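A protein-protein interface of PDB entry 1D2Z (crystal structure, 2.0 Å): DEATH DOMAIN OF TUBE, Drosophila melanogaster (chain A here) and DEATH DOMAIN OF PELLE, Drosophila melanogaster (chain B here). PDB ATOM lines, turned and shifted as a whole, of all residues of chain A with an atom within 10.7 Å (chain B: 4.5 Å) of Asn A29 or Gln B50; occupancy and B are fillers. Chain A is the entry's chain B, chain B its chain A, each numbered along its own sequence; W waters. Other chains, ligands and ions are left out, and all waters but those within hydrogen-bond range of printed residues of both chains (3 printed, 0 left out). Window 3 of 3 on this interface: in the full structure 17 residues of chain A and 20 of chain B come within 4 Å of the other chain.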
ATOM      1  N   LEU A  22      -6.358   5.613 -18.824  1.00  0.00           N
ATOM      2  CA  LEU A  22      -5.555   5.245 -19.989  1.00  0.00           C
ATOM      3  C   LEU A  22      -5.532   3.717 -20.117  1.00  0.00           C
ATOM      4  O   LEU A  22      -5.673   3.174 -21.215  1.00  0.00           O
ATOM      5  CB  LEU A  22      -4.120   5.765 -19.838  1.00  0.00           C
ATOM      6  CG  LEU A  22      -3.081   5.246 -20.842  1.00  0.00           C
ATOM      7  CD1 LEU A  22      -3.419   5.699 -22.263  1.00  0.00           C
ATOM      8  CD2 LEU A  22      -1.713   5.744 -20.447  1.00  0.00           C
ATOM      9  N   ALA A  23      -5.352   3.039 -18.985  1.00  0.00           N
ATOM     10  CA  ALA A  23      -5.298   1.575 -18.946  1.00  0.00           C
ATOM     11  C   ALA A  23      -6.540   0.919 -19.543  1.00  0.00           C
ATOM     12  O   ALA A  23      -6.426  -0.013 -20.344  1.00  0.00           O
ATOM     13  CB  ALA A  23      -5.078   1.087 -17.512  1.00  0.00           C
ATOM     14  N   LYS A  24      -7.720   1.407 -19.166  1.00  0.00           N
ATOM     15  CA  LYS A  24      -8.968   0.844 -19.682  1.00  0.00           C
ATOM     16  C   LYS A  24      -9.062   0.965 -21.201  1.00  0.00           C
ATOM     17  O   LYS A  24      -9.631   0.102 -21.875  1.00  0.00           O
ATOM     18  CB  LYS A  24     -10.185   1.486 -19.010  1.00  0.00           C
ATOM     19  CG  LYS A  24     -10.303   1.154 -17.521  1.00  0.00           C
ATOM     20  CD  LYS A  24     -10.043  -0.340 -17.251  1.00  0.00           C
ATOM     21  CE  LYS A  24     -11.089  -1.248 -17.893  1.00  0.00           C
ATOM     22  NZ  LYS A  24     -10.632  -2.674 -17.893  1.00  0.00           N
ATOM     23  N   ILE A  25      -8.479   2.030 -21.735  1.00  0.00           N
ATOM     24  CA  ILE A  25      -8.464   2.245 -23.176  1.00  0.00           C
ATOM     25  C   ILE A  25      -7.559   1.187 -23.812  1.00  0.00           C
ATOM     26  O   ILE A  25      -7.948   0.515 -24.770  1.00  0.00           O
ATOM     27  CB  ILE A  25      -7.961   3.667 -23.506  1.00  0.00           C
ATOM     28  CG1 ILE A  25      -8.927   4.697 -22.909  1.00  0.00           C
ATOM     29  CG2 ILE A  25      -7.823   3.852 -25.021  1.00  0.00           C
ATOM     30  CD1 ILE A  25      -8.523   6.124 -23.130  1.00  0.00           C
ATOM     31  N   LEU A  26      -6.376   1.000 -23.233  1.00  0.00           N
ATOM     32  CA  LEU A  26      -5.415   0.021 -23.737  1.00  0.00           C
ATOM     33  C   LEU A  26      -5.854  -1.425 -23.523  1.00  0.00           C
ATOM     34  O   LEU A  26      -5.338  -2.329 -24.180  1.00  0.00           O
ATOM     35  CB  LEU A  26      -4.034   0.251 -23.112  1.00  0.00           C
ATOM     36  CG  LEU A  26      -3.280   1.505 -23.565  1.00  0.00           C
ATOM     37  CD1 LEU A  26      -2.062   1.743 -22.677  1.00  0.00           C
ATOM     38  CD2 LEU A  26      -2.870   1.363 -25.026  1.00  0.00           C
ATOM     39  N   ASP A  27      -6.775  -1.649 -22.583  1.00  0.00           N
ATOM     40  CA  ASP A  27      -7.274  -2.999 -22.323  1.00  0.00           C
ATOM     41  C   ASP A  27      -8.103  -3.496 -23.502  1.00  0.00           C
ATOM     42  O   ASP A  27      -8.137  -4.693 -23.777  1.00  0.00           O
ATOM     43  CB  ASP A  27      -8.120  -3.053 -21.047  1.00  0.00           C
ATOM     44  CG  ASP A  27      -7.279  -3.086 -19.785  1.00  0.00           C
ATOM     45  OD1 ASP A  27      -6.144  -3.607 -19.831  1.00  0.00           O
ATOM     46  OD2 ASP A  27      -7.760  -2.598 -18.742  1.00  0.00           O
ATOM     47  N   GLU A  28      -8.776  -2.575 -24.189  1.00  0.00           N
ATOM     48  CA  GLU A  28      -9.593  -2.938 -25.343  1.00  0.00           C
ATOM     49  C   GLU A  28      -8.734  -3.525 -26.457  1.00  0.00           C
ATOM     50  O   GLU A  28      -7.677  -2.987 -26.792  1.00  0.00           O
ATOM     51  CB  GLU A  28     -10.360  -1.724 -25.871  1.00  0.00           C
ATOM     52  CG  GLU A  28     -11.439  -1.215 -24.928  1.00  0.00           C
ATOM     53  CD  GLU A  28     -12.344  -0.173 -25.567  1.00  0.00           C
ATOM     54  OE1 GLU A  28     -12.630  -0.271 -26.786  1.00  0.00           O
ATOM     55  OE2 GLU A  28     -12.785   0.741 -24.838  1.00  0.00           O
ATOM     56  N   ASN A  29      -9.181  -4.660 -26.991  1.00  0.00           N
ATOM     57  CA  ASN A  29      -8.490  -5.357 -28.074  1.00  0.00           C
ATOM     58  C   ASN A  29      -7.051  -5.715 -27.681  1.00  0.00           C
ATOM     59  O   ASN A  29      -6.180  -5.884 -28.537  1.00  0.00           O
ATOM     60  CB  ASN A  29      -8.535  -4.514 -29.362  1.00  0.00           C
ATOM     61  CG  ASN A  29      -9.966  -4.158 -29.786  1.00  0.00           C
ATOM     62  OD1 ASN A  29     -10.814  -5.039 -29.952  1.00  0.00           O
ATOM     63  ND2 ASN A  29     -10.237  -2.859 -29.962  1.00  0.00           N
ATOM     64  N   SER A  30      -6.819  -5.820 -26.372  1.00  0.00           N
ATOM     65  CA  SER A  30      -5.508  -6.161 -25.820  1.00  0.00           C
ATOM     66  C   SER A  30      -4.385  -5.293 -26.401  1.00  0.00           C
ATOM     67  O   SER A  30      -3.272  -5.773 -26.614  1.00  0.00           O
ATOM     68  CB  SER A  30      -5.215  -7.648 -26.078  1.00  0.00           C
ATOM     69  OG  SER A  30      -6.287  -8.465 -25.630  1.00  0.00           O
ATOM     70  N   CYS A  31      -4.673  -4.016 -26.636  1.00  0.00           N
ATOM     71  CA  CYS A  31      -3.684  -3.105 -27.207  1.00  0.00           C
ATOM     72  C   CYS A  31      -2.434  -2.876 -26.366  1.00  0.00           C
ATOM     73  O   CYS A  31      -1.407  -2.454 -26.893  1.00  0.00           O
ATOM     74  CB  CYS A  31      -4.326  -1.765 -27.571  1.00  0.00           C
ATOM     75  SG  CYS A  31      -5.357  -1.846 -29.051  1.00  0.00           S
ATOM     76  N   TRP A  32      -2.513  -3.172 -25.070  1.00  0.00           N
ATOM     77  CA  TRP A  32      -1.355  -3.005 -24.192  1.00  0.00           C
ATOM     78  C   TRP A  32      -0.200  -3.868 -24.695  1.00  0.00           C
ATOM     79  O   TRP A  32       0.967  -3.494 -24.562  1.00  0.00           O
ATOM     80  CB  TRP A  32      -1.700  -3.363 -22.742  1.00  0.00           C
ATOM     81  CG  TRP A  32      -2.156  -4.775 -22.542  1.00  0.00           C
ATOM     82  CD1 TRP A  32      -3.433  -5.241 -22.624  1.00  0.00           C
ATOM     83  CD2 TRP A  32      -1.337  -5.904 -22.209  1.00  0.00           C
ATOM     84  NE1 TRP A  32      -3.464  -6.587 -22.362  1.00  0.00           N
ATOM     85  CE2 TRP A  32      -2.192  -7.020 -22.102  1.00  0.00           C
ATOM     86  CE3 TRP A  32       0.036  -6.079 -21.991  1.00  0.00           C
ATOM     87  CZ2 TRP A  32      -1.724  -8.301 -21.780  1.00  0.00           C
ATOM     88  CZ3 TRP A  32       0.505  -7.354 -21.670  1.00  0.00           C
ATOM     89  CH2 TRP A  32      -0.376  -8.448 -21.569  1.00  0.00           C
ATOM     90  N   ARG A  33      -0.535  -5.015 -25.291  1.00  0.00           N
ATOM     91  CA  ARG A  33       0.480  -5.917 -25.830  1.00  0.00           C
ATOM     92  C   ARG A  33       1.246  -5.254 -26.969  1.00  0.00           C
ATOM     93  O   ARG A  33       2.468  -5.375 -27.060  1.00  0.00           O
ATOM     94  CB  ARG A  33      -0.144  -7.228 -26.327  1.00  0.00           C
ATOM     95  CG  ARG A  33      -0.805  -8.053 -25.248  1.00  0.00           C
ATOM     96  CD  ARG A  33      -1.060  -9.481 -25.711  1.00  0.00           C
ATOM     97  NE  ARG A  33      -1.876 -10.208 -24.745  1.00  0.00           N
ATOM     98  CZ  ARG A  33      -3.069 -10.729 -25.017  1.00  0.00           C
ATOM     99  NH1 ARG A  33      -3.587 -10.621 -26.235  1.00  0.00           N
ATOM    100  NH2 ARG A  33      -3.775 -11.307 -24.051  1.00  0.00           N
ATOM    101  N   LYS A  34       0.526  -4.535 -27.826  1.00  0.00           N
ATOM    102  CA  LYS A  34       1.143  -3.856 -28.958  1.00  0.00           C
ATOM    103  C   LYS A  34       2.113  -2.774 -28.491  1.00  0.00           C
ATOM    104  O   LYS A  34       3.206  -2.630 -29.041  1.00  0.00           O
ATOM    105  CB  LYS A  34       0.073  -3.255 -29.866  1.00  0.00           C
ATOM    106  CG  LYS A  34      -0.928  -4.274 -30.390  1.00  0.00           C
ATOM    107  CD  LYS A  34      -1.951  -3.612 -31.297  1.00  0.00           C
ATOM    108  CE  LYS A  34      -3.013  -4.597 -31.725  1.00  0.00           C
ATOM    109  NZ  LYS A  34      -3.921  -4.011 -32.744  1.00  0.00           N
ATOM    110  N   LEU A  35       1.708  -2.005 -27.484  1.00  0.00           N
ATOM    111  CA  LEU A  35       2.565  -0.952 -26.943  1.00  0.00           C
ATOM    112  C   LEU A  35       3.793  -1.563 -26.264  1.00  0.00           C
ATOM    113  O   LEU A  35       4.926  -1.180 -26.555  1.00  0.00           O
ATOM    114  CB  LEU A  35       1.792  -0.092 -25.933  1.00  0.00           C
ATOM    115  CG  LEU A  35       2.592   0.883 -25.052  1.00  0.00           C
ATOM    116  CD1 LEU A  35       3.305   1.930 -25.897  1.00  0.00           C
ATOM    117  CD2 LEU A  35       1.659   1.551 -24.054  1.00  0.00           C
ATOM    118  N   VAL A  71       5.630 -10.172 -21.730  1.00  0.00           N
ATOM    119  CA  VAL A  71       4.219  -9.885 -21.963  1.00  0.00           C
ATOM    120  C   VAL A  71       3.345 -10.963 -21.312  1.00  0.00           C
ATOM    121  O   VAL A  71       2.288 -10.660 -20.756  1.00  0.00           O
ATOM    122  CB  VAL A  71       3.918  -9.801 -23.478  1.00  0.00           C
ATOM    123  CG1 VAL A  71       2.442  -9.535 -23.718  1.00  0.00           C
ATOM    124  CG2 VAL A  71       4.756  -8.700 -24.121  1.00  0.00           C
ATOM    125  N   ASP A  75      -0.121 -11.440 -18.570  1.00  0.00           N
ATOM    126  CA  ASP A  75      -1.286 -12.269 -18.879  1.00  0.00           C
ATOM    127  C   ASP A  75      -1.498 -13.314 -17.782  1.00  0.00           C
ATOM    128  O   ASP A  75      -2.593 -13.428 -17.228  1.00  0.00           O
ATOM    129  CB  ASP A  75      -1.114 -12.975 -20.229  1.00  0.00           C
ATOM    130  CG  ASP A  75      -1.382 -12.058 -21.412  1.00  0.00           C
ATOM    131  OD1 ASP A  75      -2.547 -11.638 -21.590  1.00  0.00           O
ATOM    132  OD2 ASP A  75      -0.433 -11.768 -22.172  1.00  0.00           O
ATOM    133  N   LYS A  87      -5.096  -5.647 -17.418  1.00  0.00           N
ATOM    134  CA  LYS A  87      -3.743  -6.071 -17.774  1.00  0.00           C
ATOM    135  C   LYS A  87      -2.856  -4.875 -18.145  1.00  0.00           C
ATOM    136  O   LYS A  87      -1.647  -4.901 -17.909  1.00  0.00           O
ATOM    137  CB  LYS A  87      -3.786  -7.090 -18.915  1.00  0.00           C
ATOM    138  CG  LYS A  87      -4.465  -8.408 -18.529  1.00  0.00           C
ATOM    139  CD  LYS A  87      -4.483  -9.409 -19.682  1.00  0.00           C
ATOM    140  CE  LYS A  87      -5.049 -10.752 -19.227  1.00  0.00           C
ATOM    141  NZ  LYS A  87      -5.068 -11.773 -20.315  1.00  0.00           N
ATOM    142  N   SER A  88      -3.467  -3.830 -18.712  1.00  0.00           N
ATOM    143  CA  SER A  88      -2.745  -2.612 -19.094  1.00  0.00           C
ATOM    144  C   SER A  88      -2.208  -1.925 -17.846  1.00  0.00           C
ATOM    145  O   SER A  88      -1.112  -1.373 -17.858  1.00  0.00           O
ATOM    146  CB  SER A  88      -3.661  -1.636 -19.844  1.00  0.00           C
ATOM    147  OG  SER A  88      -4.097  -2.162 -21.088  1.00  0.00           O
ATOM    148  N   ALA A 117       2.439   2.724 -32.768  1.00  0.00           N
ATOM    149  CA  ALA A 117       1.646   1.493 -32.805  1.00  0.00           C
ATOM    150  C   ALA A 117       0.198   1.719 -33.275  1.00  0.00           C
ATOM    151  O   ALA A 117      -0.623   0.796 -33.251  1.00  0.00           O
ATOM    152  CB  ALA A 117       1.657   0.825 -31.431  1.00  0.00           C
ATOM    153  N   GLU A 118      -0.099   2.947 -33.692  1.00  0.00           N
ATOM    154  CA  GLU A 118      -1.430   3.340 -34.167  1.00  0.00           C
ATOM    155  C   GLU A 118      -2.549   3.164 -33.139  1.00  0.00           C
ATOM    156  O   GLU A 118      -3.704   2.902 -33.496  1.00  0.00           O
ATOM    157  CB  GLU A 118      -1.788   2.626 -35.477  1.00  0.00           C
ATOM    158  CG  GLU A 118      -0.798   2.904 -36.606  1.00  0.00           C
ATOM    159  CD  GLU A 118      -1.312   2.516 -37.988  1.00  0.00           C
ATOM    160  OE1 GLU A 118      -2.045   1.510 -38.122  1.00  0.00           O
ATOM    161  OE2 GLU A 118      -0.967   3.222 -38.953  1.00  0.00           O
ATOM    162  N   LEU A 119      -2.192   3.317 -31.865  1.00  0.00           N
ATOM    163  CA  LEU A 119      -3.142   3.212 -30.756  1.00  0.00           C
ATOM    164  C   LEU A 119      -3.683   4.632 -30.569  1.00  0.00           C
ATOM    165  O   LEU A 119      -3.411   5.302 -29.567  1.00  0.00           O
ATOM    166  CB  LEU A 119      -2.413   2.715 -29.499  1.00  0.00           C
ATOM    167  CG  LEU A 119      -1.632   1.398 -29.694  1.00  0.00           C
ATOM    168  CD1 LEU A 119      -0.929   0.986 -28.400  1.00  0.00           C
ATOM    169  CD2 LEU A 119      -2.568   0.280 -30.169  1.00  0.00           C
ATOM    170  N   PHE A 120      -4.451   5.080 -31.562  1.00  0.00           N
ATOM    171  CA  PHE A 120      -4.994   6.433 -31.571  1.00  0.00           C
ATOM    172  C   PHE A 120      -5.985   6.815 -30.491  1.00  0.00           C
ATOM    173  O   PHE A 120      -6.030   7.975 -30.089  1.00  0.00           O
ATOM    174  CB  PHE A 120      -5.496   6.797 -32.969  1.00  0.00           C
ATOM    175  CG  PHE A 120      -4.381   6.992 -33.963  1.00  0.00           C
ATOM    176  CD1 PHE A 120      -3.530   8.087 -33.859  1.00  0.00           C
ATOM    177  CD2 PHE A 120      -4.147   6.053 -34.959  1.00  0.00           C
ATOM    178  CE1 PHE A 120      -2.451   8.244 -34.735  1.00  0.00           C
ATOM    179  CE2 PHE A 120      -3.072   6.199 -35.839  1.00  0.00           C
ATOM    180  CZ  PHE A 120      -2.224   7.294 -35.727  1.00  0.00           C
ATOM    181  N   SER A 121      -6.763   5.859 -29.998  1.00  0.00           N
ATOM    182  CA  SER A 121      -7.712   6.151 -28.926  1.00  0.00           C
ATOM    183  C   SER A 121      -6.929   6.539 -27.674  1.00  0.00           C
ATOM    184  O   SER A 121      -7.273   7.496 -26.977  1.00  0.00           O
ATOM    185  CB  SER A 121      -8.580   4.937 -28.626  1.00  0.00           C
ATOM    186  OG  SER A 121      -9.893   5.141 -29.091  1.00  0.00           O
ATOM    187  N   ALA A 122      -5.862   5.794 -27.406  1.00  0.00           N
ATOM    188  CA  ALA A 122      -5.009   6.058 -26.256  1.00  0.00           C
ATOM    189  C   ALA A 122      -4.200   7.326 -26.493  1.00  0.00           C
ATOM    190  O   ALA A 122      -4.085   8.174 -25.601  1.00  0.00           O
ATOM    191  CB  ALA A 122      -4.078   4.871 -25.999  1.00  0.00           C
ATOM    192  N   ASP B  46      -4.362 -10.320 -37.919  1.00  0.00           N
ATOM    193  CA  ASP B  46      -4.816 -10.678 -36.583  1.00  0.00           C
ATOM    194  C   ASP B  46      -6.188 -10.067 -36.276  1.00  0.00           C
ATOM    195  O   ASP B  46      -7.001 -10.680 -35.581  1.00  0.00           O
ATOM    196  CB  ASP B  46      -3.798 -10.237 -35.535  1.00  0.00           C
ATOM    197  CG  ASP B  46      -3.723 -11.193 -34.367  1.00  0.00           C
ATOM    198  OD1 ASP B  46      -4.495 -11.017 -33.397  1.00  0.00           O
ATOM    199  OD2 ASP B  46      -2.899 -12.134 -34.428  1.00  0.00           O
ATOM    200  N   GLN B  47      -6.430  -8.861 -36.792  1.00  0.00           N
ATOM    201  CA  GLN B  47      -7.704  -8.163 -36.596  1.00  0.00           C
ATOM    202  C   GLN B  47      -8.808  -8.869 -37.387  1.00  0.00           C
ATOM    203  O   GLN B  47      -9.894  -9.135 -36.859  1.00  0.00           O
ATOM    204  CB  GLN B  47      -7.564  -6.695 -37.014  1.00  0.00           C
ATOM    205  CG  GLN B  47      -6.470  -5.982 -36.223  1.00  0.00           C
ATOM    206  CD  GLN B  47      -6.235  -4.549 -36.642  1.00  0.00           C
ATOM    207  OE1 GLN B  47      -5.957  -4.260 -37.811  1.00  0.00           O
ATOM    208  NE2 GLN B  47      -6.293  -3.639 -35.672  1.00  0.00           N
ATOM    209  N   VAL B  48      -8.496  -9.217 -38.636  1.00  0.00           N
ATOM    210  CA  VAL B  48      -9.417  -9.928 -39.519  1.00  0.00           C
ATOM    211  C   VAL B  48      -9.799 -11.268 -38.885  1.00  0.00           C
ATOM    212  O   VAL B  48     -10.977 -11.631 -38.835  1.00  0.00           O
ATOM    213  CB  VAL B  48      -8.769 -10.182 -40.914  1.00  0.00           C
ATOM    214  CG1 VAL B  48      -9.677 -11.038 -41.782  1.00  0.00           C
ATOM    215  CG2 VAL B  48      -8.479  -8.859 -41.610  1.00  0.00           C
ATOM    216  N   GLU B  49      -8.800 -11.981 -38.370  1.00  0.00           N
ATOM    217  CA  GLU B  49      -9.029 -13.273 -37.734  1.00  0.00           C
ATOM    218  C   GLU B  49      -9.862 -13.139 -36.463  1.00  0.00           C
ATOM    219  O   GLU B  49     -10.683 -14.000 -36.162  1.00  0.00           O
ATOM    220  CB  GLU B  49      -7.697 -13.967 -37.423  1.00  0.00           C
ATOM    221  CG  GLU B  49      -7.838 -15.375 -36.835  1.00  0.00           C
ATOM    222  CD  GLU B  49      -8.732 -16.286 -37.672  1.00  0.00           C
ATOM    223  OE1 GLU B  49      -8.638 -16.251 -38.922  1.00  0.00           O
ATOM    224  OE2 GLU B  49      -9.528 -17.041 -37.072  1.00  0.00           O
ATOM    225  N   GLN B  50      -9.648 -12.056 -35.721  1.00  0.00           N
ATOM    226  CA  GLN B  50     -10.395 -11.803 -34.492  1.00  0.00           C
ATOM    227  C   GLN B  50     -11.883 -11.655 -34.837  1.00  0.00           C
ATOM    228  O   GLN B  50     -12.740 -12.165 -34.122  1.00  0.00           O
ATOM    229  CB  GLN B  50      -9.862 -10.542 -33.799  1.00  0.00           C
ATOM    230  CG  GLN B  50     -10.595 -10.143 -32.513  1.00  0.00           C
ATOM    231  CD  GLN B  50     -10.001  -8.898 -31.869  1.00  0.00           C
ATOM    232  OE1 GLN B  50      -8.790  -8.679 -31.921  1.00  0.00           O
ATOM    233  NE2 GLN B  50     -10.851  -8.076 -31.257  1.00  0.00           N
ATOM    234  N   ILE B  51     -12.179 -10.992 -35.956  1.00  0.00           N
ATOM    235  CA  ILE B  51     -13.565 -10.811 -36.391  1.00  0.00           C
ATOM    236  C   ILE B  51     -14.143 -12.156 -36.828  1.00  0.00           C
ATOM    237  O   ILE B  51     -15.222 -12.551 -36.377  1.00  0.00           O
ATOM    238  CB  ILE B  51     -13.690  -9.823 -37.579  1.00  0.00           C
ATOM    239  CG1 ILE B  51     -13.130  -8.447 -37.195  1.00  0.00           C
ATOM    240  CG2 ILE B  51     -15.157  -9.700 -37.992  1.00  0.00           C
ATOM    241  CD1 ILE B  51     -12.945  -7.503 -38.365  1.00  0.00           C
ATOM    242  N   SER B  52     -13.425 -12.842 -37.714  1.00  0.00           N
ATOM    243  CA  SER B  52     -13.846 -14.148 -38.215  1.00  0.00           C
ATOM    244  C   SER B  52     -14.099 -15.078 -37.039  1.00  0.00           C
ATOM    245  O   SER B  52     -15.121 -15.760 -36.987  1.00  0.00           O
ATOM    246  CB  SER B  52     -12.767 -14.750 -39.125  1.00  0.00           C
ATOM    247  OG  SER B  52     -13.075 -16.092 -39.463  1.00  0.00           O
ATOM    248  N   SER B  53     -13.179 -15.050 -36.078  1.00  0.00           N
ATOM    249  CA  SER B  53     -13.254 -15.875 -34.880  1.00  0.00           C
ATOM    250  C   SER B  53     -14.518 -15.601 -34.074  1.00  0.00           C
ATOM    251  O   SER B  53     -15.219 -16.533 -33.679  1.00  0.00           O
ATOM    252  CB  SER B  53     -12.019 -15.637 -34.004  1.00  0.00           C
ATOM    253  OG  SER B  53     -12.132 -16.310 -32.764  1.00  0.00           O
ATOM    254  N   GLN B  54     -14.798 -14.325 -33.822  1.00  0.00           N
ATOM    255  CA  GLN B  54     -15.987 -13.942 -33.065  1.00  0.00           C
ATOM    256  C   GLN B  54     -17.251 -14.406 -33.764  1.00  0.00           C
ATOM    257  O   GLN B  54     -18.185 -14.867 -33.110  1.00  0.00           O
ATOM    258  CB  GLN B  54     -16.037 -12.426 -32.855  1.00  0.00           C
ATOM    259  CG  GLN B  54     -15.003 -11.906 -31.879  1.00  0.00           C
ATOM    260  CD  GLN B  54     -15.223 -12.424 -30.472  1.00  0.00           C
ATOM    261  OE1 GLN B  54     -14.404 -13.166 -29.935  1.00  0.00           O
ATOM    262  NE2 GLN B  54     -16.336 -12.037 -29.870  1.00  0.00           N
ATOM    263  N   GLU B  64     -17.885  -6.585 -34.069  1.00  0.00           N
ATOM    264  CA  GLU B  64     -16.475  -6.812 -33.774  1.00  0.00           C
ATOM    265  C   GLU B  64     -15.631  -5.872 -34.632  1.00  0.00           C
ATOM    266  O   GLU B  64     -14.620  -5.346 -34.175  1.00  0.00           O
ATOM    267  CB  GLU B  64     -16.097  -8.274 -34.021  1.00  0.00           C
ATOM    268  CG  GLU B  64     -14.711  -8.643 -33.481  1.00  0.00           C
ATOM    269  CD  GLU B  64     -14.565  -8.367 -31.987  1.00  0.00           C
ATOM    270  OE1 GLU B  64     -15.554  -8.509 -31.238  1.00  0.00           O
ATOM    271  OE2 GLU B  64     -13.457  -7.991 -31.563  1.00  0.00           O
ATOM    272  N   ASN B  67     -15.753  -2.662 -33.004  1.00  0.00           N
ATOM    273  CA  ASN B  67     -14.953  -2.722 -31.778  1.00  0.00           C
ATOM    274  C   ASN B  67     -13.478  -2.468 -32.096  1.00  0.00           C
ATOM    275  O   ASN B  67     -12.801  -1.722 -31.389  1.00  0.00           O
ATOM    276  CB  ASN B  67     -15.099  -4.090 -31.093  1.00  0.00           C
ATOM    277  CG  ASN B  67     -16.400  -4.226 -30.294  1.00  0.00           C
ATOM    278  OD1 ASN B  67     -17.041  -3.237 -29.948  1.00  0.00           O
ATOM    279  ND2 ASN B  67     -16.782  -5.461 -29.997  1.00  0.00           N
ATOM    280  N   ILE B  68     -12.994  -3.073 -33.178  1.00  0.00           N
ATOM    281  CA  ILE B  68     -11.599  -2.917 -33.588  1.00  0.00           C
ATOM    282  C   ILE B  68     -11.314  -1.564 -34.243  1.00  0.00           C
ATOM    283  O   ILE B  68     -10.499  -0.782 -33.748  1.00  0.00           O
ATOM    284  CB  ILE B  68     -11.166  -4.066 -34.553  1.00  0.00           C
ATOM    285  CG1 ILE B  68     -11.230  -5.410 -33.822  1.00  0.00           C
ATOM    286  CG2 ILE B  68      -9.750  -3.824 -35.081  1.00  0.00           C
ATOM    287  CD1 ILE B  68     -11.136  -6.629 -34.724  1.00  0.00           C
ATOM    288  N   GLN B  72      -9.891   0.908 -31.268  1.00  0.00           N
ATOM    289  CA  GLN B  72      -8.475   1.255 -31.297  1.00  0.00           C
ATOM    290  C   GLN B  72      -8.129   2.552 -32.020  1.00  0.00           C
ATOM    291  O   GLN B  72      -7.313   3.333 -31.535  1.00  0.00           O
ATOM    292  CB  GLN B  72      -7.641   0.118 -31.893  1.00  0.00           C
ATOM    293  CG  GLN B  72      -6.155   0.453 -31.965  1.00  0.00           C
ATOM    294  CD  GLN B  72      -5.325  -0.615 -32.642  1.00  0.00           C
ATOM    295  OE1 GLN B  72      -5.583  -1.820 -32.496  1.00  0.00           O
ATOM    296  NE2 GLN B  72      -4.306  -0.181 -33.379  1.00  0.00           N
HETATM  297  O   HOH W   1      -1.918  -1.236 -34.201  1.00  0.00           O
HETATM  298  O   HOH W   2      -5.950   3.035 -28.705  1.00  0.00           O
HETATM  299  O   HOH W   3      -8.786  -0.670 -28.626  1.00  0.00           O
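The side-chain amide nitrogen (NE2) of Gln B50 is in hydrogen-bond range of the side-chain amide oxygen (OD1) of Asn A29.
The backbone carbonyl oxygen (O) of Asn B67 sits at hydrogen-bond distance from the side-chain amide nitrogen (ND2) of Asn A29.
OE1 of Gln B72 sits at hydrogen-bond distance from SG of Cys A31 (3.5 Å).
The side-chain amide oxygen of Gln B72 is in hydrogen-bond range of the side-chain amino group of Lys A34, at 2.8 Å.
The side-chain amide nitrogen (NE2) of Gln B72 sits at hydrogen-bond distance from the backbone carbonyl oxygen (O) of Glu A118, at 3.1 Å.
O of Gln B72 is in hydrogen-bond range of N of Phe A120, at 3.4 Å.
N of Ser A121 lies within hydrogen-bond range of O of Gln B72, 3.0 Å away.
The side-chain carboxylate of Glu B64 lies within hydrogen-bond range of the side-chain amide nitrogen of Gln B50, 2.6 Å away.
The backbone NH (N) of Cys A31 is in hydrogen-bond range of the backbone carbonyl oxygen (O) of Leu A26 (3.1 Å).
The backbone carbonyl oxygen of Glu A28 lies within hydrogen-bond range of the side-chain sulfur of Cys A31 (3.4 Å).
Among the printed residues, pairs that only touch across the chains: Asn A29 with Ile B68 (3.9 Å), Lys A34 with Gln B47 (3.8 Å), Ala A117 with Gln B72 (3.8 Å) and Leu A119 with Gln B72 (3.7 Å).
Of the printed residues of chain B, Asn A29 touches Gln B50 (3.3 Å), Asn B67 (3.1 Å) and Ile B68 (3.9 Å).
No residue of chain A comes within 4 Å of Glu B49.
No residue of chain A comes within 4 Å of Ile B51.
No residue of chain A comes within 4 Å of Ser B53.
No residue of chain A comes within 4 Å of Gln B54.
Of chain A, only Asn A29 (3.1 Å) comes within 4 Å of Asn B67.
Of the printed residues of chain B, Ala A117 touches Gln B72 (3.8 Å).
Printed residues of chain B within 4 Å of Leu A119: Gln B72 (3.7 Å).
Ala A23 touches none of the printed residues of chain B.
Glu B64 touches none of the printed residues of chain A.
The nearest printed residue of chain B that does not touch Asn A29 is Gln B72 (4.002 Å).
The nearest residue of chain A that does not touch Gln B50 is Ser A30 (6.5 Å).
The nearest printed residue of chain B that does not touch Phe A120 is Ile B68 (8.7 Å).
Of the 13 printed residues of chain B, 5 touch a printed residue of chain A.
Printed residues of chain B that touch a printed residue of chain A: Gln B47, Gln B50, Asn B67, Ile B68 and Gln B72.
Hydrophobic or aromatic side chains of chain B within 4 Å of the printed part of chain A: Ile B68.
Along chain A the printed residues that touch a printed residue of chain B span positions 29 to 121.
Among the printed residues, 11 pairs touch across the chains.
Among the printed residues, no Asp or Glu carboxylate lies within 4 Å of a Lys or Arg side-chain nitrogen of the other chain.
Water W1 lies within hydrogen-bond range of the backbone carbonyl oxygen of Ala A117 and the side-chain amide nitrogen of Gln B72.
Water W3 lies within hydrogen-bond range of ND2 of Asn A29 (2.9 Å), O of Glu A28 (3.2 Å), N of Gln B72 (3.3 Å) and SG of Cys A31 (3.6 Å).
Water W2 lies within hydrogen-bond range of the backbone NH of Ala A122 (3.1 Å), the backbone carbonyl oxygen of Gln B72 (3.2 Å) and the backbone NH of Ser A121 (3.2 Å).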
